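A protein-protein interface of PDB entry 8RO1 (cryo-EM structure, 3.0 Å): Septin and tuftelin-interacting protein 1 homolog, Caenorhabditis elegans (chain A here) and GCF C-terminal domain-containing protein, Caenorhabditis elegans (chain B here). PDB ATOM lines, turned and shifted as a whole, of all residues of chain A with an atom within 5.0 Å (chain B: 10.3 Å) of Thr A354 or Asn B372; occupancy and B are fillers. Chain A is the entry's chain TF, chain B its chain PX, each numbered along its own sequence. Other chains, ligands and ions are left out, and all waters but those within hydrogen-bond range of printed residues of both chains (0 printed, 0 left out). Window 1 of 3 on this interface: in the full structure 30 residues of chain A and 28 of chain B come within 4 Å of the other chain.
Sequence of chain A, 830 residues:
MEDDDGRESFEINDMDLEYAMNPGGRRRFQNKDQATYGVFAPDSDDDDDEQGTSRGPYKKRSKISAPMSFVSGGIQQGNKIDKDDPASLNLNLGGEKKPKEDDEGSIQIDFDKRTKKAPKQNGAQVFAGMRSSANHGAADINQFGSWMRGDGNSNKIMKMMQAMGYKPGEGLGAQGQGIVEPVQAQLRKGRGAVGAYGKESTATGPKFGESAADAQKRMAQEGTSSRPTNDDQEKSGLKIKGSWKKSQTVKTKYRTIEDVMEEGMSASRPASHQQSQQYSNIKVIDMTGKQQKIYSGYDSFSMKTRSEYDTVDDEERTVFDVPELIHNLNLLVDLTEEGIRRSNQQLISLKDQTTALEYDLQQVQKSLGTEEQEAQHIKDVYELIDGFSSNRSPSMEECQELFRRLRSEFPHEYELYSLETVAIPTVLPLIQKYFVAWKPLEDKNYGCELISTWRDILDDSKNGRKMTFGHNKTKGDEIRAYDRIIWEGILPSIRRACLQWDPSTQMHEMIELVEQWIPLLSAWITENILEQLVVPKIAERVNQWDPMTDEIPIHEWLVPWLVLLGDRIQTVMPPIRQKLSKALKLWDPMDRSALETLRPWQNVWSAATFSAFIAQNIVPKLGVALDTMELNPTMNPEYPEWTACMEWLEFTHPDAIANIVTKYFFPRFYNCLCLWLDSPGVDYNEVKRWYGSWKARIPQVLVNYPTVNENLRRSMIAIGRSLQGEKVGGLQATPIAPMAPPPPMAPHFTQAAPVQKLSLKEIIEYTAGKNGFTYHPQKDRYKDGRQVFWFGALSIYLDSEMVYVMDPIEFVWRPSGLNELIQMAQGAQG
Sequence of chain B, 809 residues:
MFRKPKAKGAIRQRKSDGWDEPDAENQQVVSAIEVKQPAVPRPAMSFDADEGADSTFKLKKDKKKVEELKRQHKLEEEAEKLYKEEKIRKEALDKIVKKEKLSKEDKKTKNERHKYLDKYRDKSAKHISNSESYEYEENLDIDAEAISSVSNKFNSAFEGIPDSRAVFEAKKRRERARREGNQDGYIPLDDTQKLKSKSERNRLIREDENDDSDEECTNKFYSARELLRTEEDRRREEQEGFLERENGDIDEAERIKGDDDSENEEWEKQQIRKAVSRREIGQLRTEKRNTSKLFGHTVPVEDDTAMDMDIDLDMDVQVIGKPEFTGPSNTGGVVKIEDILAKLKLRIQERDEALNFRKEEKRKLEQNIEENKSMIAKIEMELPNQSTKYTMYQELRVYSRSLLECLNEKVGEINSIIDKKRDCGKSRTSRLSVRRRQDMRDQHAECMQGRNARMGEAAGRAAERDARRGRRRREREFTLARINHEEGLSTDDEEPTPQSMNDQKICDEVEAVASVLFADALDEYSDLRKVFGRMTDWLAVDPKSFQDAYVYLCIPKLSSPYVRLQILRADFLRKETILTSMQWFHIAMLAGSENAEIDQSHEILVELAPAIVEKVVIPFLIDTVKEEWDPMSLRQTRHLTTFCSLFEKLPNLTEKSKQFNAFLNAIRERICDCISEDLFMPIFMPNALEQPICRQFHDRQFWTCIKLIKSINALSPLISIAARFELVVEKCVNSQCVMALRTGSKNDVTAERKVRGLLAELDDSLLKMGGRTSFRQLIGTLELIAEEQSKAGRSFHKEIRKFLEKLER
OG1 of Thr A355 sits close to O of Lys A351 (3.4 Å). The backbone carbonyl oxygen (O) of Asn B368 sits close to the side-chain amide nitrogen (ND2) of Asn B372, at 3.2 Å. The side-chain hydroxyl (OG1) of Thr A354 sits at hydrogen-bond distance from the backbone carbonyl oxygen (O) of Leu A350.
Printed residues of chain B within 4 Å of Lys A351: Glu B380 (3.1 Å). No residue of chain B comes within 4 Å of Gln A353. Thr A354 touches just these residues of chain B: Asn B372 (3.6 Å) and Ile B376 (3.5 Å). No residue of chain B comes within 4 Å of Thr A355. Of chain B, only Ile B369 and Asn B372 come within 4 Å of Leu A357. Of chain B, only Ile B369 and Lys B373 come within 4 Å of Glu A358. Asn B372 touches just these residues of chain A: Leu A350, Thr A354 and Leu A357. Printed residues of chain A within 4 Å of Lys B373: Glu A358. Printed residues of chain A within 4 Å of Met B375: Leu A350 (3.7 Å). Printed residues of chain A within 4 Å of Glu B380: Lys A351.
Of the 17 printed residues of chain B, 6 touch a printed residue of chain A. Printed residues of chain B that touch a printed residue of chain A: Ile B369, Asn B372, Lys B373, Met B375, Ile B376 and Glu B380. Printed residues of chain A that touch a printed residue of chain B: Leu A350, Lys A351, Thr A354, Leu A357 and Glu A358. Hydrophobic or aromatic side chains of chain A that line the printed part of chain B: Leu A350 and Leu A357. Among the printed residues, Asp or Glu carboxylates within 4 Å of a Lys or Arg side-chain nitrogen of the other chain: Lys A351 with Glu B380 and Glu A358 with Lys B373.
Among the printed residues, pairs that only touch across the chains: Leu A350 with Asn B372 (3.6 Å), Leu A350 with Met B375 (3.7 Å), Leu A350 with Ile B376 (3.6 Å), Thr A354 with Asn B372 (3.6 Å), Thr A354 with Ile B376 (3.5 Å), Leu A357 with Ile B369 (3.6 Å), Leu A357 with Asn B372 (3.3 Å) and Glu A358 with Ile B369 (3.6 Å).
The side-chain amino group (NZ) of Lys B373 is in salt-bridge range of the side-chain carboxylate (OE2) of Glu A358, 2.9 Å away. The side-chain amino group (NZ) of Lys A351 lies within salt-bridge range of the side-chain carboxylate (OE2) of Glu B380 (3.2 Å).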
ATOM      1  N   SER A 349      26.655 -24.476  -7.490  1.00  0.00           N
ATOM      2  CA  SER A 349      25.956 -25.618  -8.071  1.00  0.00           C
ATOM      3  C   SER A 349      26.191 -25.719  -9.571  1.00  0.00           C
ATOM      4  O   SER A 349      26.299 -26.823 -10.117  1.00  0.00           O
ATOM      5  CB  SER A 349      24.460 -25.518  -7.780  1.00  0.00           C
ATOM      6  OG  SER A 349      23.924 -24.299  -8.263  1.00  0.00           O
ATOM      7  N   LEU A 350      26.287 -24.581 -10.253  1.00  0.00           N
ATOM      8  CA  LEU A 350      26.532 -24.612 -11.689  1.00  0.00           C
ATOM      9  C   LEU A 350      27.925 -25.138 -12.016  1.00  0.00           C
ATOM     10  O   LEU A 350      28.098 -25.871 -12.996  1.00  0.00           O
ATOM     11  CB  LEU A 350      26.316 -23.215 -12.268  1.00  0.00           C
ATOM     12  CG  LEU A 350      26.439 -23.040 -13.780  1.00  0.00           C
ATOM     13  CD1 LEU A 350      25.383 -23.865 -14.497  1.00  0.00           C
ATOM     14  CD2 LEU A 350      26.278 -21.577 -14.143  1.00  0.00           C
ATOM     15  N   LYS A 351      28.928 -24.786 -11.206  1.00  0.00           N
ATOM     16  CA  LYS A 351      30.275 -25.308 -11.428  1.00  0.00           C
ATOM     17  C   LYS A 351      30.326 -26.823 -11.285  1.00  0.00           C
ATOM     18  O   LYS A 351      30.954 -27.510 -12.099  1.00  0.00           O
ATOM     19  CB  LYS A 351      31.262 -24.671 -10.449  1.00  0.00           C
ATOM     20  CG  LYS A 351      31.670 -23.247 -10.776  1.00  0.00           C
ATOM     21  CD  LYS A 351      32.686 -22.745  -9.757  1.00  0.00           C
ATOM     22  CE  LYS A 351      33.122 -21.317 -10.036  1.00  0.00           C
ATOM     23  NZ  LYS A 351      34.212 -20.878  -9.118  1.00  0.00           N
ATOM     24  N   ASP A 352      29.692 -27.361 -10.244  1.00  0.00           N
ATOM     25  CA  ASP A 352      29.610 -28.809 -10.089  1.00  0.00           C
ATOM     26  C   ASP A 352      28.887 -29.457 -11.262  1.00  0.00           C
ATOM     27  O   ASP A 352      29.351 -30.460 -11.817  1.00  0.00           O
ATOM     28  CB  ASP A 352      28.905 -29.135  -8.775  1.00  0.00           C
ATOM     29  CG  ASP A 352      29.690 -28.669  -7.565  1.00  0.00           C
ATOM     30  OD1 ASP A 352      30.902 -28.400  -7.704  1.00  0.00           O
ATOM     31  OD2 ASP A 352      29.092 -28.559  -6.476  1.00  0.00           O
ATOM     32  N   GLN A 353      27.747 -28.889 -11.656  1.00  0.00           N
ATOM     33  CA  GLN A 353      27.014 -29.393 -12.814  1.00  0.00           C
ATOM     34  C   GLN A 353      27.849 -29.304 -14.087  1.00  0.00           C
ATOM     35  O   GLN A 353      27.792 -30.199 -14.937  1.00  0.00           O
ATOM     36  CB  GLN A 353      25.703 -28.619 -12.958  1.00  0.00           C
ATOM     37  CG  GLN A 353      24.801 -29.080 -14.085  1.00  0.00           C
ATOM     38  CD  GLN A 353      23.476 -28.347 -14.085  1.00  0.00           C
ATOM     39  OE1 GLN A 353      23.310 -27.343 -13.391  1.00  0.00           O
ATOM     40  NE2 GLN A 353      22.521 -28.848 -14.861  1.00  0.00           N
ATOM     41  N   THR A 354      28.633 -28.233 -14.233  1.00  0.00           N
ATOM     42  CA  THR A 354      29.483 -28.081 -15.411  1.00  0.00           C
ATOM     43  C   THR A 354      30.525 -29.190 -15.488  1.00  0.00           C
ATOM     44  O   THR A 354      30.762 -29.757 -16.561  1.00  0.00           O
ATOM     45  CB  THR A 354      30.155 -26.705 -15.389  1.00  0.00           C
ATOM     46  OG1 THR A 354      29.156 -25.682 -15.317  1.00  0.00           O
ATOM     47  CG2 THR A 354      31.010 -26.477 -16.635  1.00  0.00           C
ATOM     48  N   THR A 355      31.155 -29.516 -14.361  1.00  0.00           N
ATOM     49  CA  THR A 355      32.109 -30.619 -14.339  1.00  0.00           C
ATOM     50  C   THR A 355      31.429 -31.958 -14.592  1.00  0.00           C
ATOM     51  O   THR A 355      32.020 -32.844 -15.222  1.00  0.00           O
ATOM     52  CB  THR A 355      32.851 -30.645 -13.002  1.00  0.00           C
ATOM     53  OG1 THR A 355      31.911 -30.792 -11.929  1.00  0.00           O
ATOM     54  CG2 THR A 355      33.674 -29.369 -12.809  1.00  0.00           C
ATOM     55  N   ALA A 356      30.190 -32.117 -14.128  1.00  0.00           N
ATOM     56  CA  ALA A 356      29.439 -33.334 -14.415  1.00  0.00           C
ATOM     57  C   ALA A 356      29.133 -33.459 -15.902  1.00  0.00           C
ATOM     58  O   ALA A 356      29.280 -34.541 -16.483  1.00  0.00           O
ATOM     59  CB  ALA A 356      28.150 -33.355 -13.597  1.00  0.00           C
ATOM     60  N   LEU A 357      28.710 -32.366 -16.538  1.00  0.00           N
ATOM     61  CA  LEU A 357      28.469 -32.401 -17.976  1.00  0.00           C
ATOM     62  C   LEU A 357      29.753 -32.659 -18.756  1.00  0.00           C
ATOM     63  O   LEU A 357      29.740 -33.389 -19.755  1.00  0.00           O
ATOM     64  CB  LEU A 357      27.840 -31.084 -18.433  1.00  0.00           C
ATOM     65  CG  LEU A 357      26.402 -30.793 -18.001  1.00  0.00           C
ATOM     66  CD1 LEU A 357      26.067 -29.329 -18.247  1.00  0.00           C
ATOM     67  CD2 LEU A 357      25.416 -31.693 -18.733  1.00  0.00           C
ATOM     68  N   GLU A 358      30.873 -32.078 -18.319  1.00  0.00           N
ATOM     69  CA  GLU A 358      32.146 -32.353 -18.982  1.00  0.00           C
ATOM     70  C   GLU A 358      32.540 -33.816 -18.847  1.00  0.00           C
ATOM     71  O   GLU A 358      33.015 -34.427 -19.812  1.00  0.00           O
ATOM     72  CB  GLU A 358      33.253 -31.454 -18.433  1.00  0.00           C
ATOM     73  CG  GLU A 358      33.244 -30.045 -19.002  1.00  0.00           C
ATOM     74  CD  GLU A 358      34.436 -29.224 -18.546  1.00  0.00           C
ATOM     75  OE1 GLU A 358      34.868 -29.387 -17.386  1.00  0.00           O
ATOM     76  OE2 GLU A 358      34.947 -28.422 -19.354  1.00  0.00           O
ATOM     77  N   LYS B 364      24.960 -30.404 -28.702  1.00  0.00           N
ATOM     78  CA  LYS B 364      24.097 -29.855 -27.658  1.00  0.00           C
ATOM     79  C   LYS B 364      24.754 -29.899 -26.284  1.00  0.00           C
ATOM     80  O   LYS B 364      24.645 -28.946 -25.506  1.00  0.00           O
ATOM     81  CB  LYS B 364      22.769 -30.609 -27.636  1.00  0.00           C
ATOM     82  CG  LYS B 364      21.834 -30.197 -28.754  1.00  0.00           C
ATOM     83  CD  LYS B 364      20.551 -30.999 -28.739  1.00  0.00           C
ATOM     84  CE  LYS B 364      19.594 -30.532 -29.818  1.00  0.00           C
ATOM     85  NZ  LYS B 364      18.342 -31.335 -29.830  1.00  0.00           N
ATOM     86  N   LEU B 365      25.444 -30.990 -25.966  1.00  0.00           N
ATOM     87  CA  LEU B 365      26.137 -31.060 -24.687  1.00  0.00           C
ATOM     88  C   LEU B 365      27.289 -30.065 -24.631  1.00  0.00           C
ATOM     89  O   LEU B 365      27.463 -29.357 -23.632  1.00  0.00           O
ATOM     90  CB  LEU B 365      26.641 -32.484 -24.466  1.00  0.00           C
ATOM     91  CG  LEU B 365      25.588 -33.549 -24.146  1.00  0.00           C
ATOM     92  CD1 LEU B 365      26.221 -34.926 -24.186  1.00  0.00           C
ATOM     93  CD2 LEU B 365      24.934 -33.315 -22.790  1.00  0.00           C
ATOM     94  N   GLU B 366      28.075 -29.998 -25.704  1.00  0.00           N
ATOM     95  CA  GLU B 366      29.173 -29.041 -25.792  1.00  0.00           C
ATOM     96  C   GLU B 366      28.674 -27.602 -25.730  1.00  0.00           C
ATOM     97  O   GLU B 366      29.328 -26.733 -25.141  1.00  0.00           O
ATOM     98  CB  GLU B 366      29.955 -29.281 -27.082  1.00  0.00           C
ATOM     99  CG  GLU B 366      30.850 -30.511 -27.035  1.00  0.00           C
ATOM    100  CD  GLU B 366      31.530 -30.798 -28.362  1.00  0.00           C
ATOM    101  OE1 GLU B 366      31.063 -30.281 -29.400  1.00  0.00           O
ATOM    102  OE2 GLU B 366      32.528 -31.548 -28.370  1.00  0.00           O
ATOM    103  N   GLN B 367      27.513 -27.337 -26.322  1.00  0.00           N
ATOM    104  CA  GLN B 367      26.909 -26.009 -26.249  1.00  0.00           C
ATOM    105  C   GLN B 367      26.470 -25.664 -24.831  1.00  0.00           C
ATOM    106  O   GLN B 367      26.705 -24.548 -24.354  1.00  0.00           O
ATOM    107  CB  GLN B 367      25.728 -25.954 -27.219  1.00  0.00           C
ATOM    108  CG  GLN B 367      24.881 -24.696 -27.165  1.00  0.00           C
ATOM    109  CD  GLN B 367      23.918 -24.599 -28.332  1.00  0.00           C
ATOM    110  OE1 GLN B 367      23.991 -25.376 -29.285  1.00  0.00           O
ATOM    111  NE2 GLN B 367      23.008 -23.641 -28.263  1.00  0.00           N
ATOM    112  N   ASN B 368      25.817 -26.604 -24.145  1.00  0.00           N
ATOM    113  CA  ASN B 368      25.406 -26.369 -22.763  1.00  0.00           C
ATOM    114  C   ASN B 368      26.590 -26.118 -21.842  1.00  0.00           C
ATOM    115  O   ASN B 368      26.485 -25.320 -20.905  1.00  0.00           O
ATOM    116  CB  ASN B 368      24.593 -27.560 -22.259  1.00  0.00           C
ATOM    117  CG  ASN B 368      23.224 -27.637 -22.900  1.00  0.00           C
ATOM    118  OD1 ASN B 368      22.867 -26.798 -23.726  1.00  0.00           O
ATOM    119  ND2 ASN B 368      22.449 -28.647 -22.526  1.00  0.00           N
ATOM    120  N   ILE B 369      27.724 -26.772 -22.088  1.00  0.00           N
ATOM    121  CA  ILE B 369      28.896 -26.540 -21.251  1.00  0.00           C
ATOM    122  C   ILE B 369      29.453 -25.141 -21.496  1.00  0.00           C
ATOM    123  O   ILE B 369      29.836 -24.438 -20.554  1.00  0.00           O
ATOM    124  CB  ILE B 369      29.937 -27.649 -21.502  1.00  0.00           C
ATOM    125  CG1 ILE B 369      29.458 -28.949 -20.843  1.00  0.00           C
ATOM    126  CG2 ILE B 369      31.337 -27.250 -20.975  1.00  0.00           C
ATOM    127  CD1 ILE B 369      30.172 -30.202 -21.309  1.00  0.00           C
ATOM    128  N   GLU B 370      29.514 -24.719 -22.758  1.00  0.00           N
ATOM    129  CA  GLU B 370      29.970 -23.369 -23.074  1.00  0.00           C
ATOM    130  C   GLU B 370      29.009 -22.315 -22.538  1.00  0.00           C
ATOM    131  O   GLU B 370      29.439 -21.278 -22.020  1.00  0.00           O
ATOM    132  CB  GLU B 370      30.138 -23.221 -24.590  1.00  0.00           C
ATOM    133  CG  GLU B 370      30.801 -21.922 -25.063  1.00  0.00           C
ATOM    134  CD  GLU B 370      32.217 -21.747 -24.555  1.00  0.00           C
ATOM    135  OE1 GLU B 370      32.885 -22.767 -24.290  1.00  0.00           O
ATOM    136  OE2 GLU B 370      32.661 -20.586 -24.426  1.00  0.00           O
ATOM    137  N   GLU B 371      27.708 -22.574 -22.647  1.00  0.00           N
ATOM    138  CA  GLU B 371      26.709 -21.665 -22.098  1.00  0.00           C
ATOM    139  C   GLU B 371      26.833 -21.548 -20.585  1.00  0.00           C
ATOM    140  O   GLU B 371      26.723 -20.450 -20.026  1.00  0.00           O
ATOM    141  CB  GLU B 371      25.316 -22.151 -22.489  1.00  0.00           C
ATOM    142  CG  GLU B 371      24.954 -21.857 -23.936  1.00  0.00           C
ATOM    143  CD  GLU B 371      23.585 -22.382 -24.318  1.00  0.00           C
ATOM    144  OE1 GLU B 371      22.764 -22.632 -23.410  1.00  0.00           O
ATOM    145  OE2 GLU B 371      23.327 -22.541 -25.529  1.00  0.00           O
ATOM    146  N   ASN B 372      27.081 -22.665 -19.908  1.00  0.00           N
ATOM    147  CA  ASN B 372      27.252 -22.638 -18.463  1.00  0.00           C
ATOM    148  C   ASN B 372      28.528 -21.912 -18.060  1.00  0.00           C
ATOM    149  O   ASN B 372      28.526 -21.135 -17.098  1.00  0.00           O
ATOM    150  CB  ASN B 372      27.259 -24.068 -17.930  1.00  0.00           C
ATOM    151  CG  ASN B 372      25.886 -24.706 -17.960  1.00  0.00           C
ATOM    152  OD1 ASN B 372      24.871 -24.020 -18.056  1.00  0.00           O
ATOM    153  ND2 ASN B 372      25.848 -26.025 -17.868  1.00  0.00           N
ATOM    154  N   LYS B 373      29.626 -22.150 -18.778  1.00  0.00           N
ATOM    155  CA  LYS B 373      30.859 -21.413 -18.516  1.00  0.00           C
ATOM    156  C   LYS B 373      30.674 -19.914 -18.730  1.00  0.00           C
ATOM    157  O   LYS B 373      31.199 -19.103 -17.956  1.00  0.00           O
ATOM    158  CB  LYS B 373      31.986 -21.952 -19.394  1.00  0.00           C
ATOM    159  CG  LYS B 373      32.589 -23.251 -18.878  1.00  0.00           C
ATOM    160  CD  LYS B 373      33.608 -23.832 -19.848  1.00  0.00           C
ATOM    161  CE  LYS B 373      34.233 -25.108 -19.302  1.00  0.00           C
ATOM    162  NZ  LYS B 373      35.200 -25.717 -20.258  1.00  0.00           N
ATOM    163  N   SER B 374      29.933 -19.524 -19.768  1.00  0.00           N
ATOM    164  CA  SER B 374      29.633 -18.107 -19.963  1.00  0.00           C
ATOM    165  C   SER B 374      28.803 -17.563 -18.812  1.00  0.00           C
ATOM    166  O   SER B 374      29.031 -16.445 -18.339  1.00  0.00           O
ATOM    167  CB  SER B 374      28.894 -17.909 -21.283  1.00  0.00           C
ATOM    168  OG  SER B 374      28.710 -16.532 -21.559  1.00  0.00           O
ATOM    169  N   MET B 375      27.846 -18.354 -18.339  1.00  0.00           N
ATOM    170  CA  MET B 375      27.036 -17.954 -17.198  1.00  0.00           C
ATOM    171  C   MET B 375      27.887 -17.847 -15.942  1.00  0.00           C
ATOM    172  O   MET B 375      27.715 -16.918 -15.143  1.00  0.00           O
ATOM    173  CB  MET B 375      25.910 -18.964 -17.011  1.00  0.00           C
ATOM    174  CG  MET B 375      24.863 -18.585 -15.988  1.00  0.00           C
ATOM    175  SD  MET B 375      23.519 -19.789 -15.917  1.00  0.00           S
ATOM    176  CE  MET B 375      22.698 -19.519 -17.491  1.00  0.00           C
ATOM    177  N   ILE B 376      28.818 -18.787 -15.764  1.00  0.00           N
ATOM    178  CA  ILE B 376      29.760 -18.727 -14.651  1.00  0.00           C
ATOM    179  C   ILE B 376      30.583 -17.452 -14.728  1.00  0.00           C
ATOM    180  O   ILE B 376      30.747 -16.736 -13.734  1.00  0.00           O
ATOM    181  CB  ILE B 376      30.661 -19.983 -14.659  1.00  0.00           C
ATOM    182  CG1 ILE B 376      29.865 -21.210 -14.204  1.00  0.00           C
ATOM    183  CG2 ILE B 376      31.927 -19.799 -13.786  1.00  0.00           C
ATOM    184  CD1 ILE B 376      30.503 -22.558 -14.543  1.00  0.00           C
ATOM    185  N   ALA B 377      31.107 -17.151 -15.915  1.00  0.00           N
ATOM    186  CA  ALA B 377      31.913 -15.948 -16.102  1.00  0.00           C
ATOM    187  C   ALA B 377      31.135 -14.673 -15.801  1.00  0.00           C
ATOM    188  O   ALA B 377      31.685 -13.729 -15.225  1.00  0.00           O
ATOM    189  CB  ALA B 377      32.455 -15.914 -17.530  1.00  0.00           C
ATOM    190  N   LYS B 378      29.853 -14.621 -16.172  1.00  0.00           N
ATOM    191  CA  LYS B 378      29.055 -13.445 -15.841  1.00  0.00           C
ATOM    192  C   LYS B 378      28.878 -13.287 -14.336  1.00  0.00           C
ATOM    193  O   LYS B 378      29.052 -12.191 -13.795  1.00  0.00           O
ATOM    194  CB  LYS B 378      27.685 -13.544 -16.512  1.00  0.00           C
ATOM    195  CG  LYS B 378      27.679 -13.269 -18.008  1.00  0.00           C
ATOM    196  CD  LYS B 378      26.336 -13.647 -18.618  1.00  0.00           C
ATOM    197  CE  LYS B 378      26.339 -13.502 -20.127  1.00  0.00           C
ATOM    198  NZ  LYS B 378      25.066 -13.990 -20.728  1.00  0.00           N
ATOM    199  N   ILE B 379      28.554 -14.376 -13.643  1.00  0.00           N
ATOM    200  CA  ILE B 379      28.413 -14.317 -12.192  1.00  0.00           C
ATOM    201  C   ILE B 379      29.755 -14.040 -11.526  1.00  0.00           C
ATOM    202  O   ILE B 379      29.842 -13.255 -10.573  1.00  0.00           O
ATOM    203  CB  ILE B 379      27.765 -15.619 -11.676  1.00  0.00           C
ATOM    204  CG1 ILE B 379      26.313 -15.725 -12.174  1.00  0.00           C
ATOM    205  CG2 ILE B 379      27.822 -15.690 -10.137  1.00  0.00           C
ATOM    206  CD1 ILE B 379      25.690 -17.106 -12.019  1.00  0.00           C
ATOM    207  N   GLU B 380      30.820 -14.678 -12.008  1.00  0.00           N
ATOM    208  CA  GLU B 380      32.143 -14.444 -11.443  1.00  0.00           C
ATOM    209  C   GLU B 380      32.612 -13.015 -11.673  1.00  0.00           C
ATOM    210  O   GLU B 380      33.202 -12.397 -10.780  1.00  0.00           O
ATOM    211  CB  GLU B 380      33.133 -15.426 -12.061  1.00  0.00           C
ATOM    212  CG  GLU B 380      33.010 -16.839 -11.534  1.00  0.00           C
ATOM    213  CD  GLU B 380      33.976 -17.792 -12.208  1.00  0.00           C
ATOM    214  OE1 GLU B 380      34.493 -17.450 -13.290  1.00  0.00           O
ATOM    215  OE2 GLU B 380      34.197 -18.896 -11.674  1.00  0.00           O
